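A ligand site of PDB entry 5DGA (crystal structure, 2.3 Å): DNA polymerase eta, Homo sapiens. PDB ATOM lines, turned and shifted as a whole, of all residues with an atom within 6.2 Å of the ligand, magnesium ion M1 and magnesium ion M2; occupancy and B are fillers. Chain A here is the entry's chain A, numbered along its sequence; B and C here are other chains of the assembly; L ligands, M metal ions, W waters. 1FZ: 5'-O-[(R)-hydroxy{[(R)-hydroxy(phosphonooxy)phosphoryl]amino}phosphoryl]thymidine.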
ATOM      1  N   ASP A  16     -23.310  -9.969 -39.644  1.00  0.00           N
ATOM      2  CA  ASP A  16     -22.593 -10.460 -38.478  1.00  0.00           C
ATOM      3  C   ASP A  16     -23.337 -11.623 -37.806  1.00  0.00           C
ATOM      4  O   ASP A  16     -24.512 -11.509 -37.483  1.00  0.00           O
ATOM      5  CB  ASP A  16     -22.385  -9.320 -37.491  1.00  0.00           C
ATOM      6  CG  ASP A  16     -21.648  -9.748 -36.258  1.00  0.00           C
ATOM      7  OD1 ASP A  16     -22.243 -10.447 -35.445  1.00  0.00           O
ATOM      8  OD2 ASP A  16     -20.464  -9.377 -36.116  1.00  0.00           O
ATOM      9  N   MET A  17     -22.646 -12.732 -37.570  1.00  0.00           N
ATOM     10  CA  MET A  17     -23.263 -13.909 -36.966  1.00  0.00           C
ATOM     11  C   MET A  17     -23.690 -13.655 -35.520  1.00  0.00           C
ATOM     12  O   MET A  17     -23.008 -12.964 -34.774  1.00  0.00           O
ATOM     13  CB  MET A  17     -22.308 -15.106 -37.021  1.00  0.00           C
ATOM     14  CG  MET A  17     -21.569 -15.262 -38.332  1.00  0.00           C
ATOM     15  SD  MET A  17     -22.706 -15.516 -39.731  1.00  0.00           S
ATOM     16  CE  MET A  17     -23.507 -17.008 -39.223  1.00  0.00           C
ATOM     17  N   ASP A  18     -24.829 -14.206 -35.147  1.00  0.00           N
ATOM     18  CA  ASP A  18     -25.330 -14.122 -33.778  1.00  0.00           C
ATOM     19  C   ASP A  18     -24.553 -15.083 -32.882  1.00  0.00           C
ATOM     20  O   ASP A  18     -24.422 -16.261 -33.213  1.00  0.00           O
ATOM     21  CB  ASP A  18     -26.828 -14.449 -33.738  1.00  0.00           C
ATOM     22  CG  ASP A  18     -27.664 -13.525 -34.635  1.00  0.00           C
ATOM     23  OD1 ASP A  18     -27.251 -12.377 -34.859  1.00  0.00           O
ATOM     24  OD2 ASP A  18     -28.740 -13.948 -35.099  1.00  0.00           O
ATOM     25  N   CYS A  19     -24.062 -14.563 -31.758  1.00  0.00           N
ATOM     26  CA  CYS A  19     -23.304 -15.331 -30.760  1.00  0.00           C
ATOM     27  C   CYS A  19     -22.495 -16.460 -31.396  1.00  0.00           C
ATOM     28  O   CYS A  19     -22.683 -17.631 -31.071  1.00  0.00           O
ATOM     29  CB  CYS A  19     -24.250 -15.863 -29.658  1.00  0.00           C
ATOM     30  SG  CYS A  19     -25.665 -16.908 -30.164  1.00  0.00           S
ATOM     31  N   PHE A  20     -21.589 -16.093 -32.292  1.00  0.00           N
ATOM     32  CA  PHE A  20     -21.016 -17.016 -33.263  1.00  0.00           C
ATOM     33  C   PHE A  20     -20.348 -18.276 -32.690  1.00  0.00           C
ATOM     34  O   PHE A  20     -20.738 -19.389 -33.032  1.00  0.00           O
ATOM     35  CB  PHE A  20     -20.016 -16.261 -34.125  1.00  0.00           C
ATOM     36  CG  PHE A  20     -19.460 -17.072 -35.239  1.00  0.00           C
ATOM     37  CD1 PHE A  20     -20.300 -17.858 -36.028  1.00  0.00           C
ATOM     38  CD2 PHE A  20     -18.099 -17.049 -35.523  1.00  0.00           C
ATOM     39  CE1 PHE A  20     -19.803 -18.613 -37.058  1.00  0.00           C
ATOM     40  CE2 PHE A  20     -17.583 -17.799 -36.579  1.00  0.00           C
ATOM     41  CZ  PHE A  20     -18.430 -18.595 -37.346  1.00  0.00           C
ATOM     42  N   PHE A  21     -19.353 -18.118 -31.817  1.00  0.00           N
ATOM     43  CA  PHE A  21     -18.698 -19.294 -31.232  1.00  0.00           C
ATOM     44  C   PHE A  21     -19.720 -20.225 -30.555  1.00  0.00           C
ATOM     45  O   PHE A  21     -19.573 -21.445 -30.618  1.00  0.00           O
ATOM     46  CB  PHE A  21     -17.615 -18.888 -30.234  1.00  0.00           C
ATOM     47  CG  PHE A  21     -16.358 -18.317 -30.881  1.00  0.00           C
ATOM     48  CD1 PHE A  21     -16.368 -17.807 -32.172  1.00  0.00           C
ATOM     49  CD2 PHE A  21     -15.150 -18.289 -30.171  1.00  0.00           C
ATOM     50  CE1 PHE A  21     -15.217 -17.289 -32.761  1.00  0.00           C
ATOM     51  CE2 PHE A  21     -14.007 -17.778 -30.752  1.00  0.00           C
ATOM     52  CZ  PHE A  21     -14.042 -17.277 -32.054  1.00  0.00           C
ATOM     53  N   VAL A  22     -20.757 -19.665 -29.945  1.00  0.00           N
ATOM     54  CA  VAL A  22     -21.821 -20.478 -29.324  1.00  0.00           C
ATOM     55  C   VAL A  22     -22.596 -21.297 -30.393  1.00  0.00           C
ATOM     56  O   VAL A  22     -22.809 -22.511 -30.211  1.00  0.00           O
ATOM     57  CB  VAL A  22     -22.803 -19.569 -28.509  1.00  0.00           C
ATOM     58  CG1 VAL A  22     -24.060 -20.324 -28.091  1.00  0.00           C
ATOM     59  CG2 VAL A  22     -22.096 -19.001 -27.269  1.00  0.00           C
ATOM     60  N   GLN A  41     -12.765 -20.291 -22.386  1.00  0.00           N
ATOM     61  CA  GLN A  41     -11.439 -20.838 -22.652  1.00  0.00           C
ATOM     62  C   GLN A  41     -10.674 -20.892 -21.335  1.00  0.00           C
ATOM     63  O   GLN A  41     -10.782 -19.996 -20.481  1.00  0.00           O
ATOM     64  CB  GLN A  41     -10.685 -20.029 -23.721  1.00  0.00           C
ATOM     65  CG  GLN A  41     -10.242 -18.645 -23.322  1.00  0.00           C
ATOM     66  CD  GLN A  41      -9.840 -17.768 -24.521  1.00  0.00           C
ATOM     67  OE1 GLN A  41      -9.828 -18.205 -25.681  1.00  0.00           O
ATOM     68  NE2 GLN A  41      -9.533 -16.518 -24.235  1.00  0.00           N
ATOM     69  N   ILE A  51     -16.027 -16.018 -23.599  1.00  0.00           N
ATOM     70  CA  ILE A  51     -15.825 -15.186 -24.791  1.00  0.00           C
ATOM     71  C   ILE A  51     -16.993 -15.190 -25.771  1.00  0.00           C
ATOM     72  O   ILE A  51     -16.929 -14.494 -26.783  1.00  0.00           O
ATOM     73  CB  ILE A  51     -14.533 -15.571 -25.563  1.00  0.00           C
ATOM     74  CG1 ILE A  51     -14.616 -16.978 -26.137  1.00  0.00           C
ATOM     75  CG2 ILE A  51     -13.274 -15.380 -24.685  1.00  0.00           C
ATOM     76  CD1 ILE A  51     -13.349 -17.336 -26.950  1.00  0.00           C
ATOM     77  N   ALA A  52     -18.043 -15.937 -25.487  1.00  0.00           N
ATOM     78  CA  ALA A  52     -19.266 -15.838 -26.286  1.00  0.00           C
ATOM     79  C   ALA A  52     -20.467 -16.326 -25.488  1.00  0.00           C
ATOM     80  O   ALA A  52     -20.357 -17.304 -24.734  1.00  0.00           O
ATOM     81  CB  ALA A  52     -19.130 -16.631 -27.590  1.00  0.00           C
ATOM     82  N   VAL A  53     -21.605 -15.648 -25.651  1.00  0.00           N
ATOM     83  CA  VAL A  53     -22.778 -15.872 -24.806  1.00  0.00           C
ATOM     84  C   VAL A  53     -24.045 -15.939 -25.644  1.00  0.00           C
ATOM     85  O   VAL A  53     -24.304 -15.039 -26.439  1.00  0.00           O
ATOM     86  CB  VAL A  53     -22.951 -14.744 -23.767  1.00  0.00           C
ATOM     87  CG1 VAL A  53     -24.000 -15.136 -22.769  1.00  0.00           C
ATOM     88  CG2 VAL A  53     -21.643 -14.416 -23.071  1.00  0.00           C
ATOM     89  N   TYR A  55     -28.118 -15.754 -26.527  1.00  0.00           N
ATOM     90  CA  TYR A  55     -29.083 -14.740 -26.123  1.00  0.00           C
ATOM     91  C   TYR A  55     -29.920 -15.211 -24.930  1.00  0.00           C
ATOM     92  O   TYR A  55     -30.318 -14.400 -24.110  1.00  0.00           O
ATOM     93  CB  TYR A  55     -29.949 -14.316 -27.321  1.00  0.00           C
ATOM     94  CG  TYR A  55     -29.153 -13.405 -28.261  1.00  0.00           C
ATOM     95  CD1 TYR A  55     -28.229 -13.928 -29.156  1.00  0.00           C
ATOM     96  CD2 TYR A  55     -29.282 -12.013 -28.197  1.00  0.00           C
ATOM     97  CE1 TYR A  55     -27.474 -13.106 -29.987  1.00  0.00           C
ATOM     98  CE2 TYR A  55     -28.529 -11.179 -29.033  1.00  0.00           C
ATOM     99  CZ  TYR A  55     -27.624 -11.737 -29.930  1.00  0.00           C
ATOM    100  OH  TYR A  55     -26.869 -10.926 -30.771  1.00  0.00           O
ATOM    101  N   ARG A  58     -27.653 -14.312 -22.038  1.00  0.00           N
ATOM    102  CA  ARG A  58     -27.610 -12.840 -21.967  1.00  0.00           C
ATOM    103  C   ARG A  58     -28.774 -12.255 -21.154  1.00  0.00           C
ATOM    104  O   ARG A  58     -28.640 -11.192 -20.535  1.00  0.00           O
ATOM    105  CB  ARG A  58     -27.591 -12.235 -23.363  1.00  0.00           C
ATOM    106  CG  ARG A  58     -26.275 -12.375 -24.099  1.00  0.00           C
ATOM    107  CD  ARG A  58     -26.271 -11.697 -25.470  1.00  0.00           C
ATOM    108  NE  ARG A  58     -25.303 -12.320 -26.380  1.00  0.00           N
ATOM    109  CZ  ARG A  58     -24.864 -11.784 -27.508  1.00  0.00           C
ATOM    110  NH1 ARG A  58     -25.281 -10.589 -27.891  1.00  0.00           N
ATOM    111  NH2 ARG A  58     -23.995 -12.459 -28.265  1.00  0.00           N
ATOM    112  N   ARG A  64     -19.542 -11.552 -21.992  1.00  0.00           N
ATOM    113  CA  ARG A  64     -18.138 -11.786 -22.287  1.00  0.00           C
ATOM    114  C   ARG A  64     -17.209 -11.288 -21.169  1.00  0.00           C
ATOM    115  O   ARG A  64     -17.555 -10.347 -20.460  1.00  0.00           O
ATOM    116  CB  ARG A  64     -17.778 -11.080 -23.614  1.00  0.00           C
ATOM    117  CG  ARG A  64     -16.395 -11.385 -24.146  1.00  0.00           C
ATOM    118  CD  ARG A  64     -16.183 -10.844 -25.555  1.00  0.00           C
ATOM    119  NE  ARG A  64     -16.840  -9.542 -25.752  1.00  0.00           N
ATOM    120  CZ  ARG A  64     -16.240  -8.362 -25.621  1.00  0.00           C
ATOM    121  NH1 ARG A  64     -14.962  -8.280 -25.285  1.00  0.00           N
ATOM    122  NH2 ARG A  64     -16.932  -7.255 -25.835  1.00  0.00           N
ATOM    123  N   LEU A  92      -8.204 -21.872 -31.888  1.00  0.00           N
ATOM    124  CA  LEU A  92      -9.457 -21.371 -32.445  1.00  0.00           C
ATOM    125  C   LEU A  92      -9.838 -21.962 -33.807  1.00  0.00           C
ATOM    126  O   LEU A  92     -10.731 -21.457 -34.473  1.00  0.00           O
ATOM    127  CB  LEU A  92      -9.415 -19.839 -32.546  1.00  0.00           C
ATOM    128  CG  LEU A  92      -9.222 -19.117 -31.204  1.00  0.00           C
ATOM    129  CD1 LEU A  92      -9.255 -17.609 -31.375  1.00  0.00           C
ATOM    130  CD2 LEU A  92     -10.248 -19.558 -30.163  1.00  0.00           C
ATOM    131  N   SER A 116     -14.107  -9.415 -39.612  1.00  0.00           N
ATOM    132  CA  SER A 116     -13.773 -10.153 -38.395  1.00  0.00           C
ATOM    133  C   SER A 116     -13.940 -11.635 -38.655  1.00  0.00           C
ATOM    134  O   SER A 116     -14.398 -12.019 -39.729  1.00  0.00           O
ATOM    135  CB  SER A 116     -14.659  -9.719 -37.224  1.00  0.00           C
ATOM    136  OG  SER A 116     -15.876 -10.460 -37.189  1.00  0.00           O
ATOM    137  N   ILE A 117     -13.627 -12.477 -37.682  1.00  0.00           N
ATOM    138  CA  ILE A 117     -13.900 -13.891 -37.838  1.00  0.00           C
ATOM    139  C   ILE A 117     -15.388 -14.167 -38.181  1.00  0.00           C
ATOM    140  O   ILE A 117     -15.677 -15.170 -38.834  1.00  0.00           O
ATOM    141  CB  ILE A 117     -13.515 -14.693 -36.571  1.00  0.00           C
ATOM    142  CG1 ILE A 117     -13.364 -16.184 -36.926  1.00  0.00           C
ATOM    143  CG2 ILE A 117     -14.536 -14.476 -35.465  1.00  0.00           C
ATOM    144  CD1 ILE A 117     -12.929 -17.061 -35.744  1.00  0.00           C
ATOM    145  N   ASP A 118     -16.304 -13.255 -37.801  1.00  0.00           N
ATOM    146  CA  ASP A 118     -17.741 -13.542 -37.943  1.00  0.00           C
ATOM    147  C   ASP A 118     -18.547 -12.476 -38.701  1.00  0.00           C
ATOM    148  O   ASP A 118     -19.779 -12.530 -38.709  1.00  0.00           O
ATOM    149  CB  ASP A 118     -18.390 -13.799 -36.565  1.00  0.00           C
ATOM    150  CG  ASP A 118     -19.040 -12.548 -35.947  1.00  0.00           C
ATOM    151  OD1 ASP A 118     -18.421 -11.469 -35.936  1.00  0.00           O
ATOM    152  OD2 ASP A 118     -20.174 -12.687 -35.419  1.00  0.00           O
ATOM    153  N   GLU A 119     -17.887 -11.552 -39.372  1.00  0.00           N
ATOM    154  CA  GLU A 119     -18.637 -10.568 -40.167  1.00  0.00           C
ATOM    155  C   GLU A 119     -17.887 -10.093 -41.406  1.00  0.00           C
ATOM    156  O   GLU A 119     -16.663 -10.130 -41.465  1.00  0.00           O
ATOM    157  CB  GLU A 119     -19.023  -9.351 -39.290  1.00  0.00           C
ATOM    158  CG  GLU A 119     -17.877  -8.449 -38.923  1.00  0.00           C
ATOM    159  CD  GLU A 119     -18.051  -7.811 -37.553  1.00  0.00           C
ATOM    160  OE1 GLU A 119     -18.367  -6.616 -37.494  1.00  0.00           O
ATOM    161  OE2 GLU A 119     -17.857  -8.516 -36.541  1.00  0.00           O
ATOM    162  N   LYS A 227     -22.985  -1.195 -40.159  1.00  0.00           N
ATOM    163  CA  LYS A 227     -22.557  -1.805 -38.893  1.00  0.00           C
ATOM    164  C   LYS A 227     -23.478  -1.440 -37.751  1.00  0.00           C
ATOM    165  O   LYS A 227     -23.966  -2.311 -37.033  1.00  0.00           O
ATOM    166  CB  LYS A 227     -21.126  -1.397 -38.548  1.00  0.00           C
ATOM    167  CG  LYS A 227     -20.641  -1.910 -37.180  1.00  0.00           C
ATOM    168  CD  LYS A 227     -20.500  -3.437 -37.177  1.00  0.00           C
ATOM    169  CE  LYS A 227     -20.261  -3.973 -35.773  1.00  0.00           C
ATOM    170  NZ  LYS A 227     -20.015  -5.443 -35.761  1.00  0.00           N
ATOM    171  N   LYS A 234     -30.650  -7.270 -33.379  1.00  0.00           N
ATOM    172  CA  LYS A 234     -30.155  -8.618 -33.132  1.00  0.00           C
ATOM    173  C   LYS A 234     -31.046  -9.275 -32.083  1.00  0.00           C
ATOM    174  O   LYS A 234     -31.546  -8.597 -31.200  1.00  0.00           O
ATOM    175  CB  LYS A 234     -28.684  -8.579 -32.664  1.00  0.00           C
ATOM    176  CG  LYS A 234     -27.703  -8.671 -33.802  1.00  0.00           C
ATOM    177  CD  LYS A 234     -26.244  -8.533 -33.370  1.00  0.00           C
ATOM    178  CE  LYS A 234     -25.291  -9.008 -34.475  1.00  0.00           C
ATOM    179  NZ  LYS A 234     -25.155 -10.518 -34.513  1.00  0.00           N
ATOM    180  N   PRO A 235     -31.248 -10.607 -32.171  1.00  0.00           N
ATOM    181  CA  PRO A 235     -30.699 -11.575 -33.123  1.00  0.00           C
ATOM    182  C   PRO A 235     -31.628 -11.969 -34.271  1.00  0.00           C
ATOM    183  O   PRO A 235     -32.835 -11.725 -34.219  1.00  0.00           O
ATOM    184  CB  PRO A 235     -30.456 -12.801 -32.242  1.00  0.00           C
ATOM    185  CG  PRO A 235     -31.625 -12.766 -31.294  1.00  0.00           C
ATOM    186  CD  PRO A 235     -31.890 -11.289 -31.020  1.00  0.00           C
ATOM    187  P    DT B   3      -8.787  -9.354 -14.751  1.00  0.00           P
ATOM    188  OP1  DT B   3      -8.107  -8.227 -14.086  1.00  0.00           O
ATOM    189  OP2  DT B   3     -10.213  -9.649 -14.461  1.00  0.00           O
ATOM    190  O5'  DT B   3      -8.641  -9.170 -16.334  1.00  0.00           O
ATOM    191  C5'  DT B   3      -9.687  -9.608 -17.192  1.00  0.00           C
ATOM    192  C4'  DT B   3      -9.389 -10.989 -17.741  1.00  0.00           C
ATOM    193  O4'  DT B   3     -10.506 -11.426 -18.569  1.00  0.00           O
ATOM    194  C3'  DT B   3      -8.125 -11.056 -18.621  1.00  0.00           C
ATOM    195  O3'  DT B   3      -7.315 -12.210 -18.302  1.00  0.00           O
ATOM    196  C2'  DT B   3      -8.689 -11.130 -20.038  1.00  0.00           C
ATOM    197  C1'  DT B   3     -10.009 -11.869 -19.817  1.00  0.00           C
ATOM    198  N1   DT B   3     -11.005 -11.548 -20.881  1.00  0.00           N
ATOM    199  C2   DT B   3     -11.848 -12.537 -21.392  1.00  0.00           C
ATOM    200  O2   DT B   3     -11.847 -13.688 -20.996  1.00  0.00           O
ATOM    201  N3   DT B   3     -12.682 -12.113 -22.391  1.00  0.00           N
ATOM    202  C4   DT B   3     -12.773 -10.826 -22.917  1.00  0.00           C
ATOM    203  O4   DT B   3     -13.553 -10.530 -23.806  1.00  0.00           O
ATOM    204  C5   DT B   3     -11.858  -9.846 -22.343  1.00  0.00           C
ATOM    205  C7   DT B   3     -11.853  -8.430 -22.843  1.00  0.00           C
ATOM    206  C6   DT B   3     -11.032 -10.251 -21.375  1.00  0.00           C
ATOM    207  P    DA B   4      -6.000 -12.530 -19.177  1.00  0.00           P
ATOM    208  OP1  DA B   4      -5.142 -13.495 -18.455  1.00  0.00           O
ATOM    209  OP2  DA B   4      -5.468 -11.231 -19.641  1.00  0.00           O
ATOM    210  O5'  DA B   4      -6.561 -13.258 -20.482  1.00  0.00           O
ATOM    211  C5'  DA B   4      -7.181 -14.526 -20.390  1.00  0.00           C
ATOM    212  C4'  DA B   4      -7.083 -15.240 -21.729  1.00  0.00           C
ATOM    213  O4'  DA B   4      -8.106 -14.751 -22.621  1.00  0.00           O
ATOM    214  C3'  DA B   4      -5.762 -15.068 -22.463  1.00  0.00           C
ATOM    215  O3'  DA B   4      -5.450 -16.266 -23.119  1.00  0.00           O
ATOM    216  C2'  DA B   4      -6.051 -13.921 -23.446  1.00  0.00           C
ATOM    217  C1'  DA B   4      -7.522 -14.152 -23.776  1.00  0.00           C
ATOM    218  N9   DA B   4      -8.292 -12.940 -24.085  1.00  0.00           N
ATOM    219  C8   DA B   4      -8.145 -11.686 -23.541  1.00  0.00           C
ATOM    220  N7   DA B   4      -8.989 -10.796 -24.001  1.00  0.00           N
ATOM    221  C5   DA B   4      -9.766 -11.516 -24.895  1.00  0.00           C
ATOM    222  C6   DA B   4     -10.861 -11.142 -25.712  1.00  0.00           C
ATOM    223  N6   DA B   4     -11.365  -9.909 -25.758  1.00  0.00           N
ATOM    224  N1   DA B   4     -11.406 -12.104 -26.484  1.00  0.00           N
ATOM    225  C2   DA B   4     -10.902 -13.337 -26.437  1.00  0.00           C
ATOM    226  N3   DA B   4      -9.889 -13.808 -25.703  1.00  0.00           N
ATOM    227  C4   DA B   4      -9.358 -12.826 -24.953  1.00  0.00           C
ATOM    228  P   EDA B   5      -4.196 -16.363 -24.113  1.00  0.00           P
ATOM    229  OP1 EDA B   5      -3.688 -17.780 -24.053  1.00  0.00           O
ATOM    230  OP2 EDA B   5      -3.117 -15.364 -23.822  1.00  0.00           O
ATOM    231  O5' EDA B   5      -4.863 -16.096 -25.601  1.00  0.00           O
ATOM    232  N9  EDA B   5      -6.930 -13.218 -27.988  1.00  0.00           N
ATOM    233  C4  EDA B   5      -7.884 -12.357 -28.363  1.00  0.00           C
ATOM    234  N3  EDA B   5      -8.917 -12.472 -29.240  1.00  0.00           N
ATOM    235  C2  EDA B   5      -9.753 -11.427 -29.450  1.00  0.00           C
ATOM    236  N1  EDA B   5      -9.547 -10.261 -28.767  1.00  0.00           N
ATOM    237  C6  EDA B   5      -8.531 -10.134 -27.913  1.00  0.00           C
ATOM    238  C10 EDA B   5     -10.215  -9.102 -28.807  1.00  0.00           C
ATOM    239  C11 EDA B   5      -9.590  -8.257 -27.936  1.00  0.00           C
ATOM    240  N6  EDA B   5      -8.556  -8.880 -27.391  1.00  0.00           N
ATOM    241  C5  EDA B   5      -7.665 -11.207 -27.694  1.00  0.00           C
ATOM    242  N7  EDA B   5      -6.589 -11.366 -26.904  1.00  0.00           N
ATOM    243  C8  EDA B   5      -6.124 -12.626 -27.090  1.00  0.00           C
ATOM    244  C2' EDA B   5      -5.356 -14.864 -28.493  1.00  0.00           C
ATOM    245  C5' EDA B   5      -5.770 -17.084 -26.010  1.00  0.00           C
ATOM    246  C4' EDA B   5      -6.459 -16.661 -27.344  1.00  0.00           C
ATOM    247  O4' EDA B   5      -7.149 -15.596 -27.205  1.00  0.00           O
ATOM    248  C1' EDA B   5      -6.645 -14.586 -28.341  1.00  0.00           C
ATOM    249  C3' EDA B   5      -5.337 -16.347 -28.403  1.00  0.00           C
ATOM    250  O3' EDA B   5      -5.721 -16.975 -29.565  1.00  0.00           O
ATOM    251  P    DA C   7     -13.966   1.151 -31.075  1.00  0.00           P
ATOM    252  OP1  DA C   7     -15.100   1.855 -31.699  1.00  0.00           O
ATOM    253  OP2  DA C   7     -13.751   1.265 -29.609  1.00  0.00           O
ATOM    254  O5'  DA C   7     -14.112  -0.394 -31.381  1.00  0.00           O
ATOM    255  C5'  DA C   7     -14.068  -0.833 -32.719  1.00  0.00           C
ATOM    256  C4'  DA C   7     -13.777  -2.319 -32.772  1.00  0.00           C
ATOM    257  O4'  DA C   7     -12.437  -2.563 -32.309  1.00  0.00           O
ATOM    258  C3'  DA C   7     -14.677  -3.162 -31.876  1.00  0.00           C
ATOM    259  O3'  DA C   7     -15.633  -3.878 -32.669  1.00  0.00           O
ATOM    260  C2'  DA C   7     -13.712  -4.105 -31.136  1.00  0.00           C
ATOM    261  C1'  DA C   7     -12.397  -3.875 -31.849  1.00  0.00           C
ATOM    262  N9   DA C   7     -11.228  -4.018 -31.002  1.00  0.00           N
ATOM    263  C8   DA C   7     -10.832  -3.204 -29.983  1.00  0.00           C
ATOM    264  N7   DA C   7      -9.722  -3.588 -29.385  1.00  0.00           N
ATOM    265  C5   DA C   7      -9.374  -4.747 -30.064  1.00  0.00           C
ATOM    266  C6   DA C   7      -8.304  -5.636 -29.921  1.00  0.00           C
ATOM    267  N6   DA C   7      -7.344  -5.511 -28.981  1.00  0.00           N
ATOM    268  N1   DA C   7      -8.260  -6.693 -30.755  1.00  0.00           N
ATOM    269  C2   DA C   7      -9.222  -6.830 -31.682  1.00  0.00           C
ATOM    270  N3   DA C   7     -10.264  -6.060 -31.915  1.00  0.00           N
ATOM    271  C4   DA C   7     -10.290  -5.025 -31.067  1.00  0.00           C
ATOM    272  P    DT C   8     -16.949  -4.511 -31.985  1.00  0.00           P
ATOM    273  OP1  DT C   8     -18.120  -3.888 -32.625  1.00  0.00           O
ATOM    274  OP2  DT C   8     -16.786  -4.428 -30.506  1.00  0.00           O
ATOM    275  O5'  DT C   8     -16.905  -6.051 -32.444  1.00  0.00           O
HETATM  276  O2  1FZ L   1     -13.312 -14.179 -28.740  1.00  0.00           O
HETATM  277  O4  1FZ L   1     -13.573  -9.716 -27.677  1.00  0.00           O
HETATM  278  C4  1FZ L   1     -13.957 -10.670 -28.321  1.00  0.00           C
HETATM  279  C5  1FZ L   1     -15.060 -10.506 -29.274  1.00  0.00           C
HETATM  280  C6  1FZ L   1     -15.531 -11.676 -30.038  1.00  0.00           C
HETATM  281  C5M 1FZ L   1     -15.722  -9.145 -29.474  1.00  0.00           C
HETATM  282  N3  1FZ L   1     -13.350 -11.934 -28.134  1.00  0.00           N
HETATM  283  C2  1FZ L   1     -13.817 -13.095 -28.897  1.00  0.00           C
HETATM  284  N1  1FZ L   1     -14.912 -12.946 -29.855  1.00  0.00           N
HETATM  285  C1' 1FZ L   1     -15.390 -14.091 -30.605  1.00  0.00           C
HETATM  286  C2' 1FZ L   1     -16.402 -14.622 -30.042  1.00  0.00           C
HETATM  287  C3' 1FZ L   1     -17.622 -14.249 -30.891  1.00  0.00           C
HETATM  288  O3' 1FZ L   1     -18.568 -15.239 -30.907  1.00  0.00           O
HETATM  289  O4' 1FZ L   1     -15.821 -13.620 -32.075  1.00  0.00           O
HETATM  290  C4' 1FZ L   1     -17.028 -14.030 -32.279  1.00  0.00           C
HETATM  291  C5' 1FZ L   1     -17.811 -12.900 -33.015  1.00  0.00           C
HETATM  292  O5' 1FZ L   1     -17.714 -11.684 -32.261  1.00  0.00           O
HETATM  293  PA  1FZ L   1     -18.995 -10.762 -32.041  1.00  0.00           P
HETATM  294  O1A 1FZ L   1     -19.795 -10.625 -33.311  1.00  0.00           O
HETATM  295  O2A 1FZ L   1     -18.527  -9.418 -31.574  1.00  0.00           O
HETATM  296  N3A 1FZ L   1     -20.016 -11.328 -30.870  1.00  0.00           N
HETATM  297  PB  1FZ L   1     -21.051 -12.605 -31.087  1.00  0.00           P
HETATM  298  O1B 1FZ L   1     -20.639 -13.732 -30.135  1.00  0.00           O
HETATM  299  O2B 1FZ L   1     -20.991 -13.089 -32.511  1.00  0.00           O
HETATM  300  O3B 1FZ L   1     -22.488 -12.119 -30.638  1.00  0.00           O
HETATM  301  PG  1FZ L   1     -23.374 -11.045 -31.406  1.00  0.00           P
HETATM  302  O1G 1FZ L   1     -23.596  -9.873 -30.458  1.00  0.00           O
HETATM  303  O3G 1FZ L   1     -22.575 -10.598 -32.603  1.00  0.00           O
HETATM  304  O2G 1FZ L   1     -24.674 -11.673 -31.803  1.00  0.00           O
HETATM  305 MG    MG M   1     -21.472 -11.723 -33.990  1.00  0.00          MG
HETATM  306 MG    MG M   2     -18.761  -9.634 -35.035  1.00  0.00          MG
HETATM  307  O   HOH W   1     -21.836  -8.127 -33.108  1.00  0.00           O
HETATM  308  O   HOH W   2     -21.233 -13.598 -27.472  1.00  0.00           O
HETATM  309  O   HOH W   3     -19.199  -7.923 -33.819  1.00  0.00           O
HETATM  310  O   HOH W   4     -11.519 -15.509 -29.909  1.00  0.00           O
HETATM  311  O   HOH W   5     -16.801  -9.580 -34.266  1.00  0.00           O
HETATM  312  O   HOH W   6     -14.585 -11.322 -33.671  1.00  0.00           O
HETATM  313  O   HOH W   7     -25.850  -7.649 -29.456  1.00  0.00           O
HETATM  314  O   HOH W   8     -21.588  -9.225 -28.732  1.00  0.00           O
HETATM  315  O   HOH W   9     -19.422  -7.592 -29.738  1.00  0.00           O
HETATM  316  O   HOH W  10     -13.236  -6.877 -29.147  1.00  0.00           O
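OH of Tyr 55 lies within hydrogen-bond range of O2G of the ligand (2.5 Å). N1 of DA 4 of chain B is in hydrogen-bond range of a nitrogen (N3) of the ligand (2.6 Å). NH1 of Arg 58 lies within salt-bridge range of O1G of the ligand (3.2 Å). An oxygen (O2G) of the ligand is in hydrogen-bond range of the backbone NH (N) of Cys 19, at 3.0 Å. An oxygen (O2G) of the ligand is in salt-bridge range of the side-chain amino group (NZ) of Lys 234 (3.0 Å). The backbone NH (N) of Phe 20 lies within hydrogen-bond range of an oxygen (O1B) of the ligand (3.3 Å). NH1 of Arg 64 is in hydrogen-bond range of O4 of the ligand (3.1 Å). The backbone NH (N) of Phe 21 sits at hydrogen-bond distance from an oxygen (O3') of the ligand (3.1 Å).
The side-chain amino group (NZ) of Lys 227 lies close to the side-chain carboxylate (OD2) of Asp 16 (3.98 Å). N of Glu 119 sits at hydrogen-bond distance from OG of Ser 116. OE1 of Glu 119 lies within salt-bridge range of NZ of Lys 227, 2.7 Å away. The guanidinium group (NH1) of Arg 58 lies within hydrogen-bond range of the side-chain hydroxyl (OH) of Tyr 55 (3.3 Å). O4' of DA 4 of chain B sits at hydrogen-bond distance from NE2 of Gln 41 (2.8 Å). The side-chain amino group (NZ) of Lys 234 is in salt-bridge range of the side-chain carboxylate (OD1) of Asp 18, at 2.8 Å. O4 of DT 3 of chain B lies close to the guanidinium group of Arg 64 (3.0 Å). OP1 of DT 8 of chain C is in salt-bridge range of the side-chain amino group (NZ) of Lys 227 (3.98 Å).
Asp 18 touches the ligand (CA to O2G, 3.2 Å). Ile 51 touches the ligand. CB of Ala 52 touches O3' of the ligand, at 3.6 Å. CG2 of Ile 117 touches O4' of the ligand, 3.7 Å away. DT 3 of chain B touches the ligand. EDA 5 of chain B touches the ligand (C10 to O4, 3.6 Å). DT 8 of chain C touches the ligand (O5' to O2A, 3.8 Å). The nearest printed residue that does not touch the ligand is Glu 119 (4.3 Å).
Residues that only touch magnesium ion M1: Lys 234 (3.9 Å). The nearest printed residue that does not touch magnesium ion M1 is Asp 18 (4.3 Å).
Ser 116 touches magnesium ion M2 (OG to MG, 3.7 Å). The nearest printed residue that does not touch magnesium ion M2 is Lys 227 (4.4 Å).
Magnesium ion M1 is bound by O2B of the ligand (2.1 Å), OD1 of Asp 16 (2.1 Å), O3G of the ligand (2.1 Å), O1A of the ligand (2.1 Å), O of Met 17 (2.1 Å) and OD2 of Asp 118 (2.2 Å). Magnesium ion M1 has six donor atoms within binding distance.
Magnesium ion M2 is bound by the side-chain carboxylate (OD2) of Asp 16, the side-chain carboxylate (OD1) of Asp 118, the side-chain carboxylate (OE2) of Glu 119, water W5, water W3 and an oxygen (O1A) of the ligand.
Water W3 lies within hydrogen-bond range of an oxygen (O2A) of the ligand, the side-chain amino group (NZ) of Lys 227 and O5' of DT 8 of chain C. Water W5 bridges an oxygen (O5') of the ligand (3.0 Å) and the side-chain hydroxyl (OG) of Ser 116 (3.2 Å). Water W2 lies within hydrogen-bond range of an oxygen (O1B) of the ligand (2.7 Å), the backbone NH (N) of Val 53 (2.8 Å) and the guanidinium group (NH2) of Arg 58 (3.1 Å). Water W7 bridges an oxygen (O1G) of the ligand (3.3 Å) and the guanidinium group of Arg 58 (3.4 Å).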
